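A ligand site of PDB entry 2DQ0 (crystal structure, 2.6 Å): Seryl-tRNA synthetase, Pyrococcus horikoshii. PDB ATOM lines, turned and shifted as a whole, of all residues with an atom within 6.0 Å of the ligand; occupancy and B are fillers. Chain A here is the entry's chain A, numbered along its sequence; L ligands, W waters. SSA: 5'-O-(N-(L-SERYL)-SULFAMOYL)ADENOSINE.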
ATOM      1  N   PRO A 251       1.544  37.301 -24.493  1.00  0.00           N
ATOM      2  CA  PRO A 251       0.910  36.092 -25.033  1.00  0.00           C
ATOM      3  C   PRO A 251       1.955  35.035 -25.328  1.00  0.00           C
ATOM      4  O   PRO A 251       1.623  33.920 -25.721  1.00  0.00           O
ATOM      5  CB  PRO A 251       0.228  36.593 -26.308  1.00  0.00           C
ATOM      6  CG  PRO A 251       1.173  37.658 -26.770  1.00  0.00           C
ATOM      7  CD  PRO A 251       1.508  38.399 -25.495  1.00  0.00           C
ATOM      8  N   THR A 252       3.208  35.380 -25.133  1.00  0.00           N
ATOM      9  CA  THR A 252       4.339  34.496 -25.393  1.00  0.00           C
ATOM     10  C   THR A 252       5.600  35.257 -25.003  1.00  0.00           C
ATOM     11  O   THR A 252       5.638  36.470 -25.150  1.00  0.00           O
ATOM     12  CB  THR A 252       4.457  34.134 -26.887  1.00  0.00           C
ATOM     13  OG1 THR A 252       5.811  33.780 -27.187  1.00  0.00           O
ATOM     14  CG2 THR A 252       4.033  35.289 -27.753  1.00  0.00           C
ATOM     15  N   ALA A 253       6.620  34.549 -24.516  1.00  0.00           N
ATOM     16  CA  ALA A 253       7.856  35.192 -24.100  1.00  0.00           C
ATOM     17  C   ALA A 253       8.502  35.847 -25.311  1.00  0.00           C
ATOM     18  O   ALA A 253       9.331  36.746 -25.176  1.00  0.00           O
ATOM     19  CB  ALA A 253       8.815  34.173 -23.478  1.00  0.00           C
ATOM     20  N   GLU A 254       8.103  35.384 -26.496  1.00  0.00           N
ATOM     21  CA  GLU A 254       8.586  35.924 -27.767  1.00  0.00           C
ATOM     22  C   GLU A 254       8.575  37.468 -27.769  1.00  0.00           C
ATOM     23  O   GLU A 254       9.607  38.096 -28.045  1.00  0.00           O
ATOM     24  CB  GLU A 254       7.709  35.420 -28.909  1.00  0.00           C
ATOM     25  CG  GLU A 254       8.148  35.860 -30.295  1.00  0.00           C
ATOM     26  CD  GLU A 254       7.016  35.866 -31.301  1.00  0.00           C
ATOM     27  OE1 GLU A 254       6.149  34.962 -31.237  1.00  0.00           O
ATOM     28  OE2 GLU A 254       7.011  36.762 -32.181  1.00  0.00           O
ATOM     29  N   HIS A 255       7.426  38.055 -27.451  1.00  0.00           N
ATOM     30  CA  HIS A 255       7.273  39.519 -27.438  1.00  0.00           C
ATOM     31  C   HIS A 255       8.243  40.276 -26.529  1.00  0.00           C
ATOM     32  O   HIS A 255       8.882  41.209 -27.000  1.00  0.00           O
ATOM     33  CB  HIS A 255       5.836  39.925 -27.098  1.00  0.00           C
ATOM     34  CG  HIS A 255       4.829  39.412 -28.077  1.00  0.00           C
ATOM     35  ND1 HIS A 255       5.182  38.669 -29.191  1.00  0.00           N
ATOM     36  CD2 HIS A 255       3.485  39.578 -28.140  1.00  0.00           C
ATOM     37  CE1 HIS A 255       4.099  38.407 -29.898  1.00  0.00           C
ATOM     38  NE2 HIS A 255       3.053  38.947 -29.282  1.00  0.00           N
ATOM     39  N   ARG A 283      -3.705  34.659 -23.232  1.00  0.00           N
ATOM     40  CA  ARG A 283      -4.361  34.991 -24.480  1.00  0.00           C
ATOM     41  C   ARG A 283      -5.877  34.974 -24.293  1.00  0.00           C
ATOM     42  O   ARG A 283      -6.427  34.141 -23.585  1.00  0.00           O
ATOM     43  CB  ARG A 283      -3.966  34.036 -25.621  1.00  0.00           C
ATOM     44  CG  ARG A 283      -2.776  33.154 -25.334  1.00  0.00           C
ATOM     45  CD  ARG A 283      -1.566  33.430 -26.184  1.00  0.00           C
ATOM     46  NE  ARG A 283      -1.582  32.771 -27.472  1.00  0.00           N
ATOM     47  CZ  ARG A 283      -0.488  32.407 -28.147  1.00  0.00           C
ATOM     48  NH1 ARG A 283       0.707  32.645 -27.636  1.00  0.00           N
ATOM     49  NH2 ARG A 283      -0.570  31.855 -29.341  1.00  0.00           N
ATOM     50  N   GLU A 285      -8.064  34.467 -26.671  1.00  0.00           N
ATOM     51  CA  GLU A 285      -8.696  33.447 -27.508  1.00  0.00           C
ATOM     52  C   GLU A 285     -10.112  33.925 -27.805  1.00  0.00           C
ATOM     53  O   GLU A 285     -11.064  33.153 -27.717  1.00  0.00           O
ATOM     54  CB  GLU A 285      -8.737  32.095 -26.809  1.00  0.00           C
ATOM     55  CG  GLU A 285      -7.370  31.436 -26.641  1.00  0.00           C
ATOM     56  CD  GLU A 285      -6.610  31.212 -27.962  1.00  0.00           C
ATOM     57  OE1 GLU A 285      -7.247  30.958 -29.003  1.00  0.00           O
ATOM     58  OE2 GLU A 285      -5.358  31.273 -27.943  1.00  0.00           O
ATOM     59  N   ILE A 296      -7.139  21.454 -21.392  1.00  0.00           N
ATOM     60  CA  ILE A 296      -6.038  22.404 -21.399  1.00  0.00           C
ATOM     61  C   ILE A 296      -5.364  22.549 -22.745  1.00  0.00           C
ATOM     62  O   ILE A 296      -4.182  22.911 -22.844  1.00  0.00           O
ATOM     63  CB  ILE A 296      -4.973  22.020 -20.356  1.00  0.00           C
ATOM     64  CG1 ILE A 296      -4.369  20.655 -20.690  1.00  0.00           C
ATOM     65  CG2 ILE A 296      -5.575  22.039 -18.980  1.00  0.00           C
ATOM     66  CD1 ILE A 296      -3.301  20.168 -19.671  1.00  0.00           C
ATOM     67  N   PHE A 297      -6.117  22.263 -23.793  1.00  0.00           N
ATOM     68  CA  PHE A 297      -5.588  22.387 -25.138  1.00  0.00           C
ATOM     69  C   PHE A 297      -5.575  23.836 -25.608  1.00  0.00           C
ATOM     70  O   PHE A 297      -4.622  24.297 -26.234  1.00  0.00           O
ATOM     71  CB  PHE A 297      -6.441  21.575 -26.107  1.00  0.00           C
ATOM     72  CG  PHE A 297      -5.912  21.556 -27.482  1.00  0.00           C
ATOM     73  CD1 PHE A 297      -4.786  20.778 -27.800  1.00  0.00           C
ATOM     74  CD2 PHE A 297      -6.468  22.379 -28.473  1.00  0.00           C
ATOM     75  CE1 PHE A 297      -4.220  20.816 -29.087  1.00  0.00           C
ATOM     76  CE2 PHE A 297      -5.906  22.426 -29.770  1.00  0.00           C
ATOM     77  CZ  PHE A 297      -4.774  21.630 -30.067  1.00  0.00           C
ATOM     78  N   ARG A 298      -6.660  24.551 -25.328  1.00  0.00           N
ATOM     79  CA  ARG A 298      -6.776  25.943 -25.736  1.00  0.00           C
ATOM     80  C   ARG A 298      -7.386  26.708 -24.573  1.00  0.00           C
ATOM     81  O   ARG A 298      -8.611  26.773 -24.390  1.00  0.00           O
ATOM     82  CB  ARG A 298      -7.638  26.052 -27.003  1.00  0.00           C
ATOM     83  CG  ARG A 298      -7.948  27.473 -27.401  1.00  0.00           C
ATOM     84  CD  ARG A 298      -8.872  27.537 -28.594  1.00  0.00           C
ATOM     85  NE  ARG A 298      -8.151  27.329 -29.832  1.00  0.00           N
ATOM     86  CZ  ARG A 298      -8.291  26.256 -30.616  1.00  0.00           C
ATOM     87  NH1 ARG A 298      -9.136  25.292 -30.284  1.00  0.00           N
ATOM     88  NH2 ARG A 298      -7.587  26.177 -31.734  1.00  0.00           N
ATOM     89  N   VAL A 299      -6.522  27.316 -23.779  1.00  0.00           N
ATOM     90  CA  VAL A 299      -6.954  28.033 -22.609  1.00  0.00           C
ATOM     91  C   VAL A 299      -6.412  29.455 -22.559  1.00  0.00           C
ATOM     92  O   VAL A 299      -5.653  29.896 -23.431  1.00  0.00           O
ATOM     93  CB  VAL A 299      -6.486  27.286 -21.381  1.00  0.00           C
ATOM     94  CG1 VAL A 299      -7.273  25.998 -21.237  1.00  0.00           C
ATOM     95  CG2 VAL A 299      -4.977  26.955 -21.539  1.00  0.00           C
ATOM     96  N   HIS A 300      -6.809  30.171 -21.525  1.00  0.00           N
ATOM     97  CA  HIS A 300      -6.380  31.531 -21.355  1.00  0.00           C
ATOM     98  C   HIS A 300      -4.941  31.702 -20.824  1.00  0.00           C
ATOM     99  O   HIS A 300      -4.304  32.741 -21.083  1.00  0.00           O
ATOM    100  CB  HIS A 300      -7.377  32.263 -20.465  1.00  0.00           C
ATOM    101  CG  HIS A 300      -8.686  32.492 -21.147  1.00  0.00           C
ATOM    102  ND1 HIS A 300      -8.770  33.122 -22.370  1.00  0.00           N
ATOM    103  CD2 HIS A 300      -9.944  32.148 -20.799  1.00  0.00           C
ATOM    104  CE1 HIS A 300     -10.035  33.155 -22.736  1.00  0.00           C
ATOM    105  NE2 HIS A 300     -10.770  32.577 -21.808  1.00  0.00           N
ATOM    106  N   GLN A 301      -4.461  30.711 -20.059  1.00  0.00           N
ATOM    107  CA  GLN A 301      -3.097  30.771 -19.529  1.00  0.00           C
ATOM    108  C   GLN A 301      -2.402  29.423 -19.651  1.00  0.00           C
ATOM    109  O   GLN A 301      -3.006  28.373 -19.421  1.00  0.00           O
ATOM    110  CB  GLN A 301      -3.063  31.233 -18.054  1.00  0.00           C
ATOM    111  CG  GLN A 301      -3.327  30.154 -17.053  1.00  0.00           C
ATOM    112  CD  GLN A 301      -3.252  30.606 -15.578  1.00  0.00           C
ATOM    113  OE1 GLN A 301      -3.865  31.604 -15.182  1.00  0.00           O
ATOM    114  NE2 GLN A 301      -2.526  29.841 -14.764  1.00  0.00           N
ATOM    115  N   PHE A 302      -1.142  29.483 -20.051  1.00  0.00           N
ATOM    116  CA  PHE A 302      -0.290  28.306 -20.178  1.00  0.00           C
ATOM    117  C   PHE A 302       1.176  28.696 -20.078  1.00  0.00           C
ATOM    118  O   PHE A 302       1.548  29.879 -20.253  1.00  0.00           O
ATOM    119  CB  PHE A 302      -0.512  27.573 -21.496  1.00  0.00           C
ATOM    120  CG  PHE A 302      -0.209  28.396 -22.717  1.00  0.00           C
ATOM    121  CD1 PHE A 302      -1.163  29.272 -23.236  1.00  0.00           C
ATOM    122  CD2 PHE A 302       1.006  28.255 -23.380  1.00  0.00           C
ATOM    123  CE1 PHE A 302      -0.899  29.998 -24.408  1.00  0.00           C
ATOM    124  CE2 PHE A 302       1.270  28.981 -24.552  1.00  0.00           C
ATOM    125  CZ  PHE A 302       0.319  29.848 -25.061  1.00  0.00           C
ATOM    126  N   LYS A 304       5.145  28.281 -21.315  1.00  0.00           N
ATOM    127  CA  LYS A 304       5.903  27.985 -22.525  1.00  0.00           C
ATOM    128  C   LYS A 304       7.382  28.360 -22.490  1.00  0.00           C
ATOM    129  O   LYS A 304       7.745  29.462 -22.136  1.00  0.00           O
ATOM    130  CB  LYS A 304       5.242  28.641 -23.734  1.00  0.00           C
ATOM    131  CG  LYS A 304       5.911  28.307 -25.041  1.00  0.00           C
ATOM    132  CD  LYS A 304       5.062  28.741 -26.243  1.00  0.00           C
ATOM    133  CE  LYS A 304       4.718  30.239 -26.169  1.00  0.00           C
ATOM    134  NZ  LYS A 304       5.943  31.105 -26.100  1.00  0.00           N
ATOM    135  N   GLU A 306      10.370  29.204 -24.622  1.00  0.00           N
ATOM    136  CA  GLU A 306      10.509  29.755 -25.974  1.00  0.00           C
ATOM    137  C   GLU A 306      11.912  30.007 -26.502  1.00  0.00           C
ATOM    138  O   GLU A 306      12.774  30.518 -25.784  1.00  0.00           O
ATOM    139  CB  GLU A 306       9.724  31.069 -26.023  1.00  0.00           C
ATOM    140  CG  GLU A 306       9.816  31.834 -27.326  1.00  0.00           C
ATOM    141  CD  GLU A 306       8.777  31.391 -28.313  1.00  0.00           C
ATOM    142  OE1 GLU A 306       8.275  30.266 -28.158  1.00  0.00           O
ATOM    143  OE2 GLU A 306       8.474  32.171 -29.247  1.00  0.00           O
ATOM    144  N   ASP A 357       5.257  24.088 -38.362  1.00  0.00           N
ATOM    145  CA  ASP A 357       4.526  23.691 -37.168  1.00  0.00           C
ATOM    146  C   ASP A 357       4.775  22.221 -36.874  1.00  0.00           C
ATOM    147  O   ASP A 357       4.967  21.402 -37.781  1.00  0.00           O
ATOM    148  CB  ASP A 357       3.013  23.867 -37.351  1.00  0.00           C
ATOM    149  CG  ASP A 357       2.531  25.293 -37.139  1.00  0.00           C
ATOM    150  OD1 ASP A 357       3.360  26.231 -37.152  1.00  0.00           O
ATOM    151  OD2 ASP A 357       1.306  25.475 -36.997  1.00  0.00           O
ATOM    152  N   GLU A 370      -1.426  20.973 -33.663  1.00  0.00           N
ATOM    153  CA  GLU A 370      -0.306  21.897 -33.487  1.00  0.00           C
ATOM    154  C   GLU A 370       0.165  21.828 -32.061  1.00  0.00           C
ATOM    155  O   GLU A 370      -0.642  21.892 -31.122  1.00  0.00           O
ATOM    156  CB  GLU A 370      -0.697  23.347 -33.770  1.00  0.00           C
ATOM    157  CG  GLU A 370       0.428  24.333 -33.433  1.00  0.00           C
ATOM    158  CD  GLU A 370       0.069  25.777 -33.674  1.00  0.00           C
ATOM    159  OE1 GLU A 370       0.898  26.660 -33.350  1.00  0.00           O
ATOM    160  OE2 GLU A 370      -1.032  26.049 -34.209  1.00  0.00           O
ATOM    161  N   VAL A 371       1.475  21.749 -31.902  1.00  0.00           N
ATOM    162  CA  VAL A 371       2.068  21.652 -30.592  1.00  0.00           C
ATOM    163  C   VAL A 371       3.262  22.631 -30.493  1.00  0.00           C
ATOM    164  O   VAL A 371       3.715  22.937 -29.404  1.00  0.00           O
ATOM    165  CB  VAL A 371       2.430  20.169 -30.339  1.00  0.00           C
ATOM    166  CG1 VAL A 371       3.873  19.856 -30.772  1.00  0.00           C
ATOM    167  CG2 VAL A 371       2.130  19.824 -28.906  1.00  0.00           C
ATOM    168  N   VAL A 372       3.746  23.099 -31.644  1.00  0.00           N
ATOM    169  CA  VAL A 372       4.836  24.087 -31.693  1.00  0.00           C
ATOM    170  C   VAL A 372       4.848  24.829 -33.024  1.00  0.00           C
ATOM    171  O   VAL A 372       4.409  24.307 -34.048  1.00  0.00           O
ATOM    172  CB  VAL A 372       6.290  23.495 -31.440  1.00  0.00           C
ATOM    173  CG1 VAL A 372       6.243  22.010 -31.312  1.00  0.00           C
ATOM    174  CG2 VAL A 372       7.248  23.899 -32.563  1.00  0.00           C
ATOM    175  N   SER A 373       5.361  26.048 -32.992  1.00  0.00           N
ATOM    176  CA  SER A 373       5.469  26.893 -34.171  1.00  0.00           C
ATOM    177  C   SER A 373       6.857  27.512 -34.212  1.00  0.00           C
ATOM    178  O   SER A 373       7.379  27.974 -33.186  1.00  0.00           O
ATOM    179  CB  SER A 373       4.412  27.993 -34.105  1.00  0.00           C
ATOM    180  OG  SER A 373       3.688  28.046 -35.323  1.00  0.00           O
ATOM    181  N   ALA A 374       7.472  27.488 -35.393  1.00  0.00           N
ATOM    182  CA  ALA A 374       8.809  28.073 -35.616  1.00  0.00           C
ATOM    183  C   ALA A 374       8.703  29.057 -36.787  1.00  0.00           C
ATOM    184  O   ALA A 374       8.388  28.670 -37.897  1.00  0.00           O
ATOM    185  CB  ALA A 374       9.818  26.984 -35.929  1.00  0.00           C
ATOM    186  N   SER A 375       8.980  30.322 -36.525  1.00  0.00           N
ATOM    187  CA  SER A 375       8.880  31.336 -37.565  1.00  0.00           C
ATOM    188  C   SER A 375      10.178  32.075 -37.861  1.00  0.00           C
ATOM    189  O   SER A 375      11.017  32.288 -36.988  1.00  0.00           O
ATOM    190  CB  SER A 375       7.848  32.393 -37.149  1.00  0.00           C
ATOM    191  OG  SER A 375       6.609  31.798 -36.797  1.00  0.00           O
ATOM    192  N   ASN A 404      11.647  32.923 -33.944  1.00  0.00           N
ATOM    193  CA  ASN A 404      11.137  32.392 -32.698  1.00  0.00           C
ATOM    194  C   ASN A 404      10.550  31.015 -32.947  1.00  0.00           C
ATOM    195  O   ASN A 404      10.159  30.666 -34.070  1.00  0.00           O
ATOM    196  CB  ASN A 404      10.089  33.324 -32.070  1.00  0.00           C
ATOM    197  CG  ASN A 404       8.817  33.404 -32.875  1.00  0.00           C
ATOM    198  OD1 ASN A 404       8.004  32.475 -32.877  1.00  0.00           O
ATOM    199  ND2 ASN A 404       8.617  34.513 -33.571  1.00  0.00           N
ATOM    200  N   SER A 405      10.531  30.221 -31.901  1.00  0.00           N
ATOM    201  CA  SER A 405       9.994  28.895 -32.012  1.00  0.00           C
ATOM    202  C   SER A 405       9.700  28.323 -30.656  1.00  0.00           C
ATOM    203  O   SER A 405      10.433  28.522 -29.680  1.00  0.00           O
ATOM    204  CB  SER A 405      10.985  27.976 -32.729  1.00  0.00           C
ATOM    205  OG  SER A 405      10.515  26.634 -32.785  1.00  0.00           O
ATOM    206  N   THR A 406       8.594  27.607 -30.603  1.00  0.00           N
ATOM    207  CA  THR A 406       8.232  26.954 -29.378  1.00  0.00           C
ATOM    208  C   THR A 406       9.315  25.931 -29.093  1.00  0.00           C
ATOM    209  O   THR A 406       9.826  25.303 -30.020  1.00  0.00           O
ATOM    210  CB  THR A 406       6.916  26.169 -29.553  1.00  0.00           C
ATOM    211  OG1 THR A 406       5.954  26.995 -30.211  1.00  0.00           O
ATOM    212  CG2 THR A 406       6.374  25.715 -28.199  1.00  0.00           C
ATOM    213  N   ALA A 407       9.677  25.768 -27.828  1.00  0.00           N
ATOM    214  CA  ALA A 407      10.586  24.690 -27.457  1.00  0.00           C
ATOM    215  C   ALA A 407       9.497  23.749 -26.923  1.00  0.00           C
ATOM    216  O   ALA A 407       9.245  22.702 -27.479  1.00  0.00           O
ATOM    217  CB  ALA A 407      11.532  25.090 -26.358  1.00  0.00           C
ATOM    218  N   ALA A 409       5.426  24.115 -25.122  1.00  0.00           N
ATOM    219  CA  ALA A 409       4.343  24.846 -24.500  1.00  0.00           C
ATOM    220  C   ALA A 409       3.775  23.669 -23.687  1.00  0.00           C
ATOM    221  O   ALA A 409       3.240  22.720 -24.255  1.00  0.00           O
ATOM    222  CB  ALA A 409       3.366  25.350 -25.567  1.00  0.00           C
ATOM    223  N   SER A 411       1.148  23.100 -21.802  1.00  0.00           N
ATOM    224  CA  SER A 411      -0.268  22.785 -21.985  1.00  0.00           C
ATOM    225  C   SER A 411      -0.437  21.615 -22.982  1.00  0.00           C
ATOM    226  O   SER A 411      -0.848  20.516 -22.615  1.00  0.00           O
ATOM    227  CB  SER A 411      -0.993  24.022 -22.523  1.00  0.00           C
ATOM    228  OG  SER A 411      -0.290  24.555 -23.636  1.00  0.00           O
ATOM    229  N   ARG A 412      -0.088  21.874 -24.235  1.00  0.00           N
ATOM    230  CA  ARG A 412      -0.243  20.853 -25.258  1.00  0.00           C
ATOM    231  C   ARG A 412       0.745  19.702 -25.196  1.00  0.00           C
ATOM    232  O   ARG A 412       0.478  18.654 -25.769  1.00  0.00           O
ATOM    233  CB  ARG A 412      -0.212  21.492 -26.629  1.00  0.00           C
ATOM    234  CG  ARG A 412      -1.348  22.499 -26.731  1.00  0.00           C
ATOM    235  CD  ARG A 412      -1.538  22.996 -28.102  1.00  0.00           C
ATOM    236  NE  ARG A 412      -2.740  23.784 -28.170  1.00  0.00           N
ATOM    237  CZ  ARG A 412      -3.160  24.401 -29.256  1.00  0.00           C
ATOM    238  NH1 ARG A 412      -4.291  25.098 -29.211  1.00  0.00           N
ATOM    239  NH2 ARG A 412      -2.449  24.331 -30.387  1.00  0.00           N
HETATM  240  N10 SSA L   1       6.117  32.788 -30.133  1.00  0.00           N
HETATM  241  CA  SSA L   1       5.548  31.763 -31.040  1.00  0.00           C
HETATM  242  CB  SSA L   1       6.385  30.516 -31.032  1.00  0.00           C
HETATM  243  OG  SSA L   1       6.249  29.775 -29.811  1.00  0.00           O
HETATM  244  C9  SSA L   1       4.124  31.367 -30.693  1.00  0.00           C
HETATM  245  O9  SSA L   1       3.585  31.771 -29.667  1.00  0.00           O
HETATM  246  N8  SSA L   1       3.494  30.574 -31.569  1.00  0.00           N
HETATM  247  S1  SSA L   1       2.006  30.055 -31.257  1.00  0.00           S
HETATM  248  O1S SSA L   1       1.177  31.257 -31.201  1.00  0.00           O
HETATM  249  O2S SSA L   1       1.724  29.025 -32.255  1.00  0.00           O
HETATM  250  O5' SSA L   1       2.106  29.421 -29.830  1.00  0.00           O
HETATM  251  C5' SSA L   1       3.028  28.373 -29.601  1.00  0.00           C
HETATM  252  C4' SSA L   1       2.367  27.169 -29.010  1.00  0.00           C
HETATM  253  O4' SSA L   1       1.792  27.481 -27.738  1.00  0.00           O
HETATM  254  C3' SSA L   1       1.230  26.531 -29.777  1.00  0.00           C
HETATM  255  O3' SSA L   1       1.743  25.752 -30.840  1.00  0.00           O
HETATM  256  C2' SSA L   1       0.661  25.646 -28.685  1.00  0.00           C
HETATM  257  O2' SSA L   1       1.448  24.521 -28.381  1.00  0.00           O
HETATM  258  C1' SSA L   1       0.682  26.628 -27.506  1.00  0.00           C
HETATM  259  N9  SSA L   1      -0.506  27.478 -27.416  1.00  0.00           N
HETATM  260  C8  SSA L   1      -0.847  28.592 -28.167  1.00  0.00           C
HETATM  261  N7  SSA L   1      -1.987  29.121 -27.815  1.00  0.00           N
HETATM  262  C5  SSA L   1      -2.437  28.313 -26.783  1.00  0.00           C
HETATM  263  C6  SSA L   1      -3.615  28.335 -25.986  1.00  0.00           C
HETATM  264  N6  SSA L   1      -4.568  29.249 -26.133  1.00  0.00           N
HETATM  265  N1  SSA L   1      -3.753  27.384 -25.019  1.00  0.00           N
HETATM  266  C2  SSA L   1      -2.768  26.460 -24.870  1.00  0.00           C
HETATM  267  N3  SSA L   1      -1.615  26.345 -25.570  1.00  0.00           N
HETATM  268  C4  SSA L   1      -1.526  27.297 -26.522  1.00  0.00           C
HETATM  269  O   HOH W   1       6.605  30.761 -34.456  1.00  0.00           O
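Water W1 lies within hydrogen-bond range of OG of Ser 375 (2.6 Å), OD1 of Asn 404 (2.7 Å) and O of Ser 373 (3.2 Å).
The side-chain carboxylate (OE1) of Glu 306 is in salt-bridge range of the side-chain amino group (NZ) of Lys 304 (3.2 Å).
The backbone carbonyl oxygen (O) of Pro 251 sits at hydrogen-bond distance from the guanidinium group (NH1) of Arg 283 (2.5 Å).
The backbone carbonyl oxygen of Ser 373 lies close to the side-chain hydroxyl of Ser 405 (3.4 Å).
The backbone NH (N) of Glu 254 lies within hydrogen-bond range of the side-chain hydroxyl (OG1) of Thr 252 (2.9 Å).
O of Arg 283 lies within hydrogen-bond range of ND1 of His 300 (2.8 Å).
OG1 of Thr 252 is in hydrogen-bond range of NZ of Lys 304 (2.9 Å).
ND2 of Asn 404 lies close to OE2 of Glu 254 (3.1 Å).
N of Ser 375 sits at hydrogen-bond distance from O of Asn 404, 2.7 Å away.
The backbone carbonyl oxygen (O) of Val 371 is in hydrogen-bond range of an oxygen (O2') of the ligand, 2.9 Å away.
N10 of the ligand is in salt-bridge range of OE2 of Glu 306 (2.6 Å).
N of Val 299 lies within hydrogen-bond range of N1 of the ligand (3.0 Å).
O3' of the ligand lies within hydrogen-bond range of OE1 of Glu 370 (2.8 Å).
The side-chain hydroxyl (OG1) of Thr 406 is in hydrogen-bond range of an oxygen (OG) of the ligand.
An oxygen (O1S) of the ligand sits at hydrogen-bond distance from the guanidinium group (NH2) of Arg 283, at 2.6 Å.
An oxygen (OG) of the ligand is in hydrogen-bond range of the backbone NH (N) of Thr 406, at 3.3 Å.
OE2 of Glu 285 is in hydrogen-bond range of N6 of the ligand.
OG1 of Thr 252 sits at hydrogen-bond distance from N10 of the ligand.
N6 of the ligand is in hydrogen-bond range of O of Val 299 (3.0 Å).
A nitrogen (N3) of the ligand sits at hydrogen-bond distance from the side-chain hydroxyl (OG) of Ser 411 (2.9 Å).
An oxygen (O3') of the ligand lies within hydrogen-bond range of the backbone NH (N) of Val 372 (3.4 Å).
N10 of the ligand sits close to OD1 of Asn 404 (3.3 Å).
OE1 of Glu 254 lies within salt-bridge range of N10 of the ligand, at 2.4 Å.
The backbone carbonyl oxygen (O) of Phe 297 lies close to a nitrogen (N1) of the ligand, 3.4 Å away.
CA of Arg 298 touches N1 of the ligand (3.4 Å).
CE1 of Phe 302 touches C5 of the ligand (3.3 Å).
Lys 304 touches the ligand.
Ser 373 touches the ligand (CB to O2S, 3.4 Å).
C of Ser 405 touches OG of the ligand, 3.8 Å away.
CB of Ala 409 touches O4' of the ligand (3.4 Å).
Arg 412 touches the ligand.
Within 4 Å of the ligand: Thr 252, Glu 254, Arg 283, Glu 285, Phe 297, Arg 298, Val 299, Phe 302, Lys 304, Glu 306, Glu 370, Val 371, Val 372, Ser 373, Asn 404, Ser 405, Thr 406, Ala 409, Ser 411 and Arg 412.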
